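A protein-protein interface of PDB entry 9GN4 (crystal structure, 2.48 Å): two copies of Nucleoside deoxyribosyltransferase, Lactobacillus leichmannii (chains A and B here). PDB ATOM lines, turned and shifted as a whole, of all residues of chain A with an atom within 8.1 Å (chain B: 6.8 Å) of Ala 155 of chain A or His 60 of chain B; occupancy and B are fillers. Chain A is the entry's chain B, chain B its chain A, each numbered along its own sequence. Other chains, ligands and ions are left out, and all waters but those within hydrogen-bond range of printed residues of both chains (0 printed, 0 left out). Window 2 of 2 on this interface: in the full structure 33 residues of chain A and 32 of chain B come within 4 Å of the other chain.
Hydrophobic or aromatic side chains of chain A that line the printed part of chain B: Leu 124, Trp 127 and Ala 155.
Along chain A the printed residues that touch a printed residue of chain B span positions 124 to 157.
Among the printed residues, 9 pairs touch across the chains.
Among the printed residues, Asp or Glu carboxylates within 4 Å of a Lys or Arg side-chain nitrogen of the other chain: Glu 153 of chain A with Lys 62 of chain B (3.1 Å).
Ala 155 of chain A touches two residues of chain B.
Of the printed residues of chain B, Glu 153 of chain A touches Lys 62 (3.1 Å).
Of the printed residues of chain A, Val 52 of chain B touches Tyr 157.
Tyr 58 of chain B touches none of the printed residues of chain A.
The nearest residue of chain A that does not touch His 60 of chain B is Gly 119 of chain A (4.8 Å).
The nearest printed residue of chain B that does not touch Val 156 of chain A is Val 52 of chain B (4.3 Å).
No position is printed for both chains.
Of the 9 pairs that touch across the chains among the printed residues, none has its exchanged pair printed and touching as well.
The backbone carbonyl oxygen of Leu 59 of chain B is in hydrogen-bond range of the backbone NH of Val 156 of chain A.
The side-chain amino group of Lys 62 of chain B is in salt-bridge range of the side-chain carboxylate of Glu 153 of chain A.
Among the printed residues, pairs that only touch across the chains: Gly 154 of chain A with His 60 of chain B (3.3 Å), Ala 155 of chain A with Leu 59 of chain B (3.4 Å), Leu 124 of chain A with Ala 65 of chain B (3.4 Å), Tyr 157 of chain A with Val 52 of chain B (3.4 Å), Trp 127 of chain A with Ala 65 of chain B (3.5 Å), Ala 155 of chain A with His 60 of chain B (3.6 Å) and Trp 127 of chain A with Lys 62 of chain B (3.8 Å).
OH of Tyr 118 of chain A sits at hydrogen-bond distance from N of Glu 153 of chain A.
The backbone carbonyl oxygen of Gly 119 of chain A lies within hydrogen-bond range of the backbone NH of Ala 155 of chain A.
N of Ile 122 of chain A sits at hydrogen-bond distance from O of Ala 155 of chain A (3.0 Å).
The backbone carbonyl oxygen of Ile 122 of chain A lies within hydrogen-bond range of the backbone NH of Tyr 157 of chain A (3.0 Å).
The side-chain amide nitrogen (ND2) of Asn 123 of chain A lies within hydrogen-bond range of the side-chain hydroxyl (OH) of Tyr 157 of chain A.
OXT of Tyr 157 of chain A lies within hydrogen-bond range of N of Leu 124 of chain A (3.0 Å).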
ATOM      1  N   PRO A  88      25.033  -1.595   2.734  1.00  0.00           N
ATOM      2  CA  PRO A  88      25.448  -0.208   2.579  1.00  0.00           C
ATOM      3  C   PRO A  88      26.953   0.065   2.587  1.00  0.00           C
ATOM      4  O   PRO A  88      27.430   0.971   1.875  1.00  0.00           O
ATOM      5  CB  PRO A  88      24.717   0.476   3.740  1.00  0.00           C
ATOM      6  CG  PRO A  88      23.461  -0.356   3.887  1.00  0.00           C
ATOM      7  CD  PRO A  88      23.963  -1.745   3.736  1.00  0.00           C
ATOM      8  N   GLU A  91      28.734  -1.865  -1.200  1.00  0.00           N
ATOM      9  CA  GLU A  91      27.840  -1.741  -2.336  1.00  0.00           C
ATOM     10  C   GLU A  91      28.481  -2.357  -3.583  1.00  0.00           C
ATOM     11  O   GLU A  91      29.682  -2.290  -3.737  1.00  0.00           O
ATOM     12  CB  GLU A  91      27.462  -0.282  -2.517  1.00  0.00           C
ATOM     13  CG  GLU A  91      26.603   0.271  -1.383  1.00  0.00           C
ATOM     14  CD  GLU A  91      26.467   1.783  -1.520  1.00  0.00           C
ATOM     15  OE1 GLU A  91      27.509   2.487  -1.498  1.00  0.00           O
ATOM     16  OE2 GLU A  91      25.330   2.261  -1.688  1.00  0.00           O
ATOM     17  N   ILE A 113      17.884  -4.722   3.365  1.00  0.00           N
ATOM     18  CA  ILE A 113      19.092  -4.384   4.098  1.00  0.00           C
ATOM     19  C   ILE A 113      19.039  -5.040   5.479  1.00  0.00           C
ATOM     20  O   ILE A 113      18.007  -5.008   6.154  1.00  0.00           O
ATOM     21  CB  ILE A 113      19.226  -2.861   4.211  1.00  0.00           C
ATOM     22  CG1 ILE A 113      19.286  -2.239   2.829  1.00  0.00           C
ATOM     23  CG2 ILE A 113      20.432  -2.474   5.076  1.00  0.00           C
ATOM     24  CD1 ILE A 113      19.344  -0.725   2.812  1.00  0.00           C
ATOM     25  N   ASP A 117      22.065  -2.698   9.706  1.00  0.00           N
ATOM     26  CA  ASP A 117      22.576  -1.734   8.741  1.00  0.00           C
ATOM     27  C   ASP A 117      21.507  -0.758   8.269  1.00  0.00           C
ATOM     28  O   ASP A 117      21.860   0.274   7.716  1.00  0.00           O
ATOM     29  CB  ASP A 117      23.210  -2.464   7.568  1.00  0.00           C
ATOM     30  CG  ASP A 117      24.521  -3.166   7.886  1.00  0.00           C
ATOM     31  OD1 ASP A 117      25.184  -2.743   8.868  1.00  0.00           O
ATOM     32  OD2 ASP A 117      24.871  -4.110   7.155  1.00  0.00           O
ATOM     33  N   TYR A 118      20.223  -1.077   8.490  1.00  0.00           N
ATOM     34  CA  TYR A 118      19.148  -0.253   7.970  1.00  0.00           C
ATOM     35  C   TYR A 118      19.227   1.157   8.566  1.00  0.00           C
ATOM     36  O   TYR A 118      19.107   1.346   9.772  1.00  0.00           O
ATOM     37  CB  TYR A 118      17.775  -0.891   8.214  1.00  0.00           C
ATOM     38  CG  TYR A 118      16.657  -0.251   7.398  1.00  0.00           C
ATOM     39  CD1 TYR A 118      16.079   0.958   7.768  1.00  0.00           C
ATOM     40  CD2 TYR A 118      16.158  -0.872   6.258  1.00  0.00           C
ATOM     41  CE1 TYR A 118      15.052   1.527   7.023  1.00  0.00           C
ATOM     42  CE2 TYR A 118      15.151  -0.302   5.493  1.00  0.00           C
ATOM     43  CZ  TYR A 118      14.602   0.904   5.871  1.00  0.00           C
ATOM     44  OH  TYR A 118      13.612   1.448   5.093  1.00  0.00           O
ATOM     45  N   GLY A 119      19.329   2.156   7.688  1.00  0.00           N
ATOM     46  CA  GLY A 119      19.446   3.558   8.069  1.00  0.00           C
ATOM     47  C   GLY A 119      20.756   4.177   7.595  1.00  0.00           C
ATOM     48  O   GLY A 119      20.875   5.398   7.511  1.00  0.00           O
ATOM     49  N   LYS A 120      21.740   3.325   7.304  1.00  0.00           N
ATOM     50  CA  LYS A 120      23.048   3.767   6.831  1.00  0.00           C
ATOM     51  C   LYS A 120      22.946   4.305   5.401  1.00  0.00           C
ATOM     52  O   LYS A 120      22.065   3.933   4.627  1.00  0.00           O
ATOM     53  CB  LYS A 120      24.081   2.632   6.845  1.00  0.00           C
ATOM     54  CG  LYS A 120      24.409   2.127   8.223  1.00  0.00           C
ATOM     55  CD  LYS A 120      25.759   1.441   8.323  1.00  0.00           C
ATOM     56  CE  LYS A 120      25.597   0.187   9.089  1.00  0.00           C
ATOM     57  NZ  LYS A 120      26.868  -0.451   9.410  1.00  0.00           N
ATOM     58  N   PRO A 121      23.848   5.220   5.012  1.00  0.00           N
ATOM     59  CA  PRO A 121      23.743   5.851   3.709  1.00  0.00           C
ATOM     60  C   PRO A 121      23.872   4.846   2.573  1.00  0.00           C
ATOM     61  O   PRO A 121      24.693   3.932   2.653  1.00  0.00           O
ATOM     62  CB  PRO A 121      24.916   6.841   3.671  1.00  0.00           C
ATOM     63  CG  PRO A 121      25.451   6.919   5.099  1.00  0.00           C
ATOM     64  CD  PRO A 121      25.017   5.655   5.793  1.00  0.00           C
ATOM     65  N   ILE A 122      23.062   5.048   1.525  1.00  0.00           N
ATOM     66  CA  ILE A 122      23.177   4.306   0.280  1.00  0.00           C
ATOM     67  C   ILE A 122      23.240   5.312  -0.864  1.00  0.00           C
ATOM     68  O   ILE A 122      22.807   6.446  -0.759  1.00  0.00           O
ATOM     69  CB  ILE A 122      22.006   3.338   0.091  1.00  0.00           C
ATOM     70  CG1 ILE A 122      20.663   4.091  -0.117  1.00  0.00           C
ATOM     71  CG2 ILE A 122      21.964   2.372   1.272  1.00  0.00           C
ATOM     72  CD1 ILE A 122      19.471   3.200  -0.440  1.00  0.00           C
ATOM     73  N   ASN A 123      23.818   4.862  -1.963  1.00  0.00           N
ATOM     74  CA  ASN A 123      23.985   5.656  -3.163  1.00  0.00           C
ATOM     75  C   ASN A 123      22.644   6.207  -3.653  1.00  0.00           C
ATOM     76  O   ASN A 123      21.642   5.501  -3.697  1.00  0.00           O
ATOM     77  CB  ASN A 123      24.612   4.780  -4.235  1.00  0.00           C
ATOM     78  CG  ASN A 123      25.121   5.607  -5.379  1.00  0.00           C
ATOM     79  OD1 ASN A 123      24.330   6.111  -6.190  1.00  0.00           O
ATOM     80  ND2 ASN A 123      26.434   5.769  -5.413  1.00  0.00           N
ATOM     81  N   LEU A 124      22.644   7.465  -4.086  1.00  0.00           N
ATOM     82  CA  LEU A 124      21.462   8.109  -4.656  1.00  0.00           C
ATOM     83  C   LEU A 124      20.770   7.211  -5.675  1.00  0.00           C
ATOM     84  O   LEU A 124      19.552   7.120  -5.669  1.00  0.00           O
ATOM     85  CB  LEU A 124      21.849   9.417  -5.331  1.00  0.00           C
ATOM     86  CG  LEU A 124      20.727  10.139  -6.084  1.00  0.00           C
ATOM     87  CD1 LEU A 124      19.666  10.582  -5.106  1.00  0.00           C
ATOM     88  CD2 LEU A 124      21.247  11.342  -6.875  1.00  0.00           C
ATOM     89  N   TRP A 127      19.011   4.314  -4.154  1.00  0.00           N
ATOM     90  CA  TRP A 127      17.821   4.902  -3.579  1.00  0.00           C
ATOM     91  C   TRP A 127      16.736   5.133  -4.637  1.00  0.00           C
ATOM     92  O   TRP A 127      15.587   4.759  -4.438  1.00  0.00           O
ATOM     93  CB  TRP A 127      18.228   6.203  -2.874  1.00  0.00           C
ATOM     94  CG  TRP A 127      17.081   6.943  -2.253  1.00  0.00           C
ATOM     95  CD1 TRP A 127      16.626   6.845  -0.969  1.00  0.00           C
ATOM     96  CD2 TRP A 127      16.265   7.939  -2.893  1.00  0.00           C
ATOM     97  NE1 TRP A 127      15.582   7.702  -0.772  1.00  0.00           N
ATOM     98  CE2 TRP A 127      15.334   8.384  -1.930  1.00  0.00           C
ATOM     99  CE3 TRP A 127      16.235   8.499  -4.168  1.00  0.00           C
ATOM    100  CZ2 TRP A 127      14.399   9.373  -2.205  1.00  0.00           C
ATOM    101  CZ3 TRP A 127      15.291   9.468  -4.447  1.00  0.00           C
ATOM    102  CH2 TRP A 127      14.379   9.893  -3.485  1.00  0.00           C
ATOM    103  N   TYR A 152      13.146   4.676   1.299  1.00  0.00           N
ATOM    104  CA  TYR A 152      14.063   4.307   2.373  1.00  0.00           C
ATOM    105  C   TYR A 152      14.038   5.344   3.492  1.00  0.00           C
ATOM    106  O   TYR A 152      14.150   6.531   3.212  1.00  0.00           O
ATOM    107  CB  TYR A 152      15.477   4.268   1.788  1.00  0.00           C
ATOM    108  CG  TYR A 152      16.637   3.809   2.665  1.00  0.00           C
ATOM    109  CD1 TYR A 152      16.539   2.704   3.500  1.00  0.00           C
ATOM    110  CD2 TYR A 152      17.846   4.492   2.652  1.00  0.00           C
ATOM    111  CE1 TYR A 152      17.615   2.276   4.260  1.00  0.00           C
ATOM    112  CE2 TYR A 152      18.941   4.054   3.373  1.00  0.00           C
ATOM    113  CZ  TYR A 152      18.830   2.940   4.173  1.00  0.00           C
ATOM    114  OH  TYR A 152      19.939   2.593   4.887  1.00  0.00           O
ATOM    115  N   GLU A 153      13.892   4.877   4.733  1.00  0.00           N
ATOM    116  CA  GLU A 153      13.983   5.726   5.915  1.00  0.00           C
ATOM    117  C   GLU A 153      15.441   5.642   6.364  1.00  0.00           C
ATOM    118  O   GLU A 153      15.800   4.814   7.210  1.00  0.00           O
ATOM    119  CB  GLU A 153      12.960   5.356   7.000  1.00  0.00           C
ATOM    120  CG  GLU A 153      11.512   5.747   6.666  1.00  0.00           C
ATOM    121  CD  GLU A 153      11.183   6.994   5.804  1.00  0.00           C
ATOM    122  OE1 GLU A 153      11.659   8.151   6.058  1.00  0.00           O
ATOM    123  OE2 GLU A 153      10.394   6.801   4.827  1.00  0.00           O
ATOM    124  N   GLY A 154      16.274   6.476   5.730  1.00  0.00           N
ATOM    125  CA  GLY A 154      17.714   6.339   5.812  1.00  0.00           C
ATOM    126  C   GLY A 154      18.418   7.359   4.923  1.00  0.00           C
ATOM    127  O   GLY A 154      17.786   8.137   4.229  1.00  0.00           O
ATOM    128  N   ALA A 155      19.741   7.384   5.000  1.00  0.00           N
ATOM    129  CA  ALA A 155      20.506   8.446   4.374  1.00  0.00           C
ATOM    130  C   ALA A 155      20.878   8.059   2.942  1.00  0.00           C
ATOM    131  O   ALA A 155      21.001   6.880   2.633  1.00  0.00           O
ATOM    132  CB  ALA A 155      21.720   8.700   5.231  1.00  0.00           C
ATOM    133  N   VAL A 156      21.017   9.046   2.060  1.00  0.00           N
ATOM    134  CA  VAL A 156      21.664   8.808   0.784  1.00  0.00           C
ATOM    135  C   VAL A 156      22.950   9.617   0.756  1.00  0.00           C
ATOM    136  O   VAL A 156      23.037  10.618   1.458  1.00  0.00           O
ATOM    137  CB  VAL A 156      20.767   9.210  -0.391  1.00  0.00           C
ATOM    138  CG1 VAL A 156      19.318   8.811  -0.140  1.00  0.00           C
ATOM    139  CG2 VAL A 156      20.902  10.709  -0.615  1.00  0.00           C
ATOM    140  N   TYR A 157      23.917   9.189  -0.072  1.00  0.00           N
ATOM    141  CA  TYR A 157      25.079   9.997  -0.422  1.00  0.00           C
ATOM    142  C   TYR A 157      25.101  10.241  -1.958  1.00  0.00           C
ATOM    143  O   TYR A 157      25.856  11.163  -2.314  1.00  0.00           O
ATOM    144  CB  TYR A 157      26.340   9.317   0.116  1.00  0.00           C
ATOM    145  CG  TYR A 157      26.729   8.036  -0.604  1.00  0.00           C
ATOM    146  CD1 TYR A 157      27.467   8.090  -1.774  1.00  0.00           C
ATOM    147  CD2 TYR A 157      26.411   6.785  -0.091  1.00  0.00           C
ATOM    148  CE1 TYR A 157      27.867   6.938  -2.430  1.00  0.00           C
ATOM    149  CE2 TYR A 157      26.801   5.620  -0.737  1.00  0.00           C
ATOM    150  CZ  TYR A 157      27.539   5.700  -1.906  1.00  0.00           C
ATOM    151  OH  TYR A 157      27.865   4.573  -2.592  1.00  0.00           O
ATOM    152  OXT TYR A 157      24.398   9.561  -2.757  1.00  0.00           O
ATOM    153  N   VAL B  52      25.760  16.959  -1.228  1.00  0.00           N
ATOM    154  CA  VAL B  52      25.340  16.474   0.073  1.00  0.00           C
ATOM    155  C   VAL B  52      26.543  16.341   1.015  1.00  0.00           C
ATOM    156  O   VAL B  52      26.354  16.316   2.218  1.00  0.00           O
ATOM    157  CB  VAL B  52      24.542  15.155  -0.040  1.00  0.00           C
ATOM    158  CG1 VAL B  52      25.422  13.958  -0.359  1.00  0.00           C
ATOM    159  CG2 VAL B  52      23.694  14.871   1.201  1.00  0.00           C
ATOM    160  N   PRO B  56      25.471  18.322   4.627  1.00  0.00           N
ATOM    161  CA  PRO B  56      24.867  17.098   5.134  1.00  0.00           C
ATOM    162  C   PRO B  56      23.444  17.202   5.708  1.00  0.00           C
ATOM    163  O   PRO B  56      22.800  16.179   5.999  1.00  0.00           O
ATOM    164  CB  PRO B  56      25.843  16.637   6.205  1.00  0.00           C
ATOM    165  CG  PRO B  56      27.130  17.377   5.935  1.00  0.00           C
ATOM    166  CD  PRO B  56      26.716  18.666   5.327  1.00  0.00           C
ATOM    167  N   GLU B  57      22.932  18.427   5.847  1.00  0.00           N
ATOM    168  CA  GLU B  57      21.520  18.605   6.129  1.00  0.00           C
ATOM    169  C   GLU B  57      20.661  17.980   5.021  1.00  0.00           C
ATOM    170  O   GLU B  57      19.492  17.713   5.247  1.00  0.00           O
ATOM    171  CB  GLU B  57      21.133  20.063   6.406  1.00  0.00           C
ATOM    172  CG  GLU B  57      21.303  21.063   5.266  1.00  0.00           C
ATOM    173  CD  GLU B  57      22.645  21.773   5.209  1.00  0.00           C
ATOM    174  OE1 GLU B  57      23.621  21.202   5.743  1.00  0.00           O
ATOM    175  OE2 GLU B  57      22.730  22.882   4.621  1.00  0.00           O
ATOM    176  N   TYR B  58      21.222  17.746   3.835  1.00  0.00           N
ATOM    177  CA  TYR B  58      20.457  17.172   2.742  1.00  0.00           C
ATOM    178  C   TYR B  58      20.530  15.642   2.688  1.00  0.00           C
ATOM    179  O   TYR B  58      19.929  15.064   1.801  1.00  0.00           O
ATOM    180  CB  TYR B  58      20.878  17.776   1.409  1.00  0.00           C
ATOM    181  CG  TYR B  58      20.393  19.196   1.209  1.00  0.00           C
ATOM    182  CD1 TYR B  58      21.101  20.282   1.716  1.00  0.00           C
ATOM    183  CD2 TYR B  58      19.218  19.453   0.510  1.00  0.00           C
ATOM    184  CE1 TYR B  58      20.676  21.589   1.505  1.00  0.00           C
ATOM    185  CE2 TYR B  58      18.768  20.751   0.298  1.00  0.00           C
ATOM    186  CZ  TYR B  58      19.492  21.818   0.816  1.00  0.00           C
ATOM    187  OH  TYR B  58      19.041  23.094   0.620  1.00  0.00           O
ATOM    188  N   LEU B  59      21.153  14.980   3.666  1.00  0.00           N
ATOM    189  CA  LEU B  59      21.364  13.535   3.620  1.00  0.00           C
ATOM    190  C   LEU B  59      20.033  12.763   3.669  1.00  0.00           C
ATOM    191  O   LEU B  59      19.996  11.579   3.296  1.00  0.00           O
ATOM    192  CB  LEU B  59      22.255  13.077   4.780  1.00  0.00           C
ATOM    193  CG  LEU B  59      23.782  13.181   4.631  1.00  0.00           C
ATOM    194  CD1 LEU B  59      24.450  12.778   5.947  1.00  0.00           C
ATOM    195  CD2 LEU B  59      24.368  12.335   3.506  1.00  0.00           C
ATOM    196  N   HIS B  60      18.977  13.386   4.229  1.00  0.00           N
ATOM    197  CA  HIS B  60      17.672  12.746   4.346  1.00  0.00           C
ATOM    198  C   HIS B  60      16.608  13.577   3.630  1.00  0.00           C
ATOM    199  O   HIS B  60      15.428  13.249   3.774  1.00  0.00           O
ATOM    200  CB  HIS B  60      17.228  12.508   5.812  1.00  0.00           C
ATOM    201  CG  HIS B  60      18.054  11.531   6.594  1.00  0.00           C
ATOM    202  ND1 HIS B  60      19.211  11.915   7.246  1.00  0.00           N
ATOM    203  CD2 HIS B  60      17.936  10.205   6.822  1.00  0.00           C
ATOM    204  CE1 HIS B  60      19.767  10.865   7.853  1.00  0.00           C
ATOM    205  NE2 HIS B  60      19.009   9.813   7.622  1.00  0.00           N
ATOM    206  N   ASP B  61      17.000  14.627   2.867  1.00  0.00           N
ATOM    207  CA  ASP B  61      16.024  15.365   2.072  1.00  0.00           C
ATOM    208  C   ASP B  61      15.560  14.553   0.838  1.00  0.00           C
ATOM    209  O   ASP B  61      16.305  14.309  -0.117  1.00  0.00           O
ATOM    210  CB  ASP B  61      16.516  16.772   1.758  1.00  0.00           C
ATOM    211  CG  ASP B  61      15.552  17.650   0.958  1.00  0.00           C
ATOM    212  OD1 ASP B  61      14.471  17.168   0.559  1.00  0.00           O
ATOM    213  OD2 ASP B  61      15.878  18.817   0.717  1.00  0.00           O
ATOM    214  N   LYS B  62      14.288  14.159   0.847  1.00  0.00           N
ATOM    215  CA  LYS B  62      13.719  13.304  -0.184  1.00  0.00           C
ATOM    216  C   LYS B  62      13.471  14.067  -1.489  1.00  0.00           C
ATOM    217  O   LYS B  62      13.466  13.471  -2.570  1.00  0.00           O
ATOM    218  CB  LYS B  62      12.401  12.693   0.309  1.00  0.00           C
ATOM    219  CG  LYS B  62      12.578  11.584   1.342  1.00  0.00           C
ATOM    220  CD  LYS B  62      11.223  10.928   1.610  1.00  0.00           C
ATOM    221  CE  LYS B  62      11.252   9.833   2.626  1.00  0.00           C
ATOM    222  NZ  LYS B  62      11.704  10.336   3.926  1.00  0.00           N
ATOM    223  N   VAL B  63      13.285  15.384  -1.384  1.00  0.00           N
ATOM    224  CA  VAL B  63      13.047  16.232  -2.541  1.00  0.00           C
ATOM    225  C   VAL B  63      14.345  16.420  -3.325  1.00  0.00           C
ATOM    226  O   VAL B  63      14.340  16.299  -4.555  1.00  0.00           O
ATOM    227  CB  VAL B  63      12.495  17.585  -2.059  1.00  0.00           C
ATOM    228  CG1 VAL B  63      12.469  18.640  -3.175  1.00  0.00           C
ATOM    229  CG2 VAL B  63      11.120  17.427  -1.394  1.00  0.00           C
ATOM    230  N   ALA B  65      16.880  14.418  -3.246  1.00  0.00           N
ATOM    231  CA  ALA B  65      17.202  13.119  -3.792  1.00  0.00           C
ATOM    232  C   ALA B  65      16.360  12.810  -5.030  1.00  0.00           C
ATOM    233  O   ALA B  65      16.878  12.307  -6.033  1.00  0.00           O
ATOM    234  CB  ALA B  65      17.011  12.071  -2.740  1.00  0.00           C
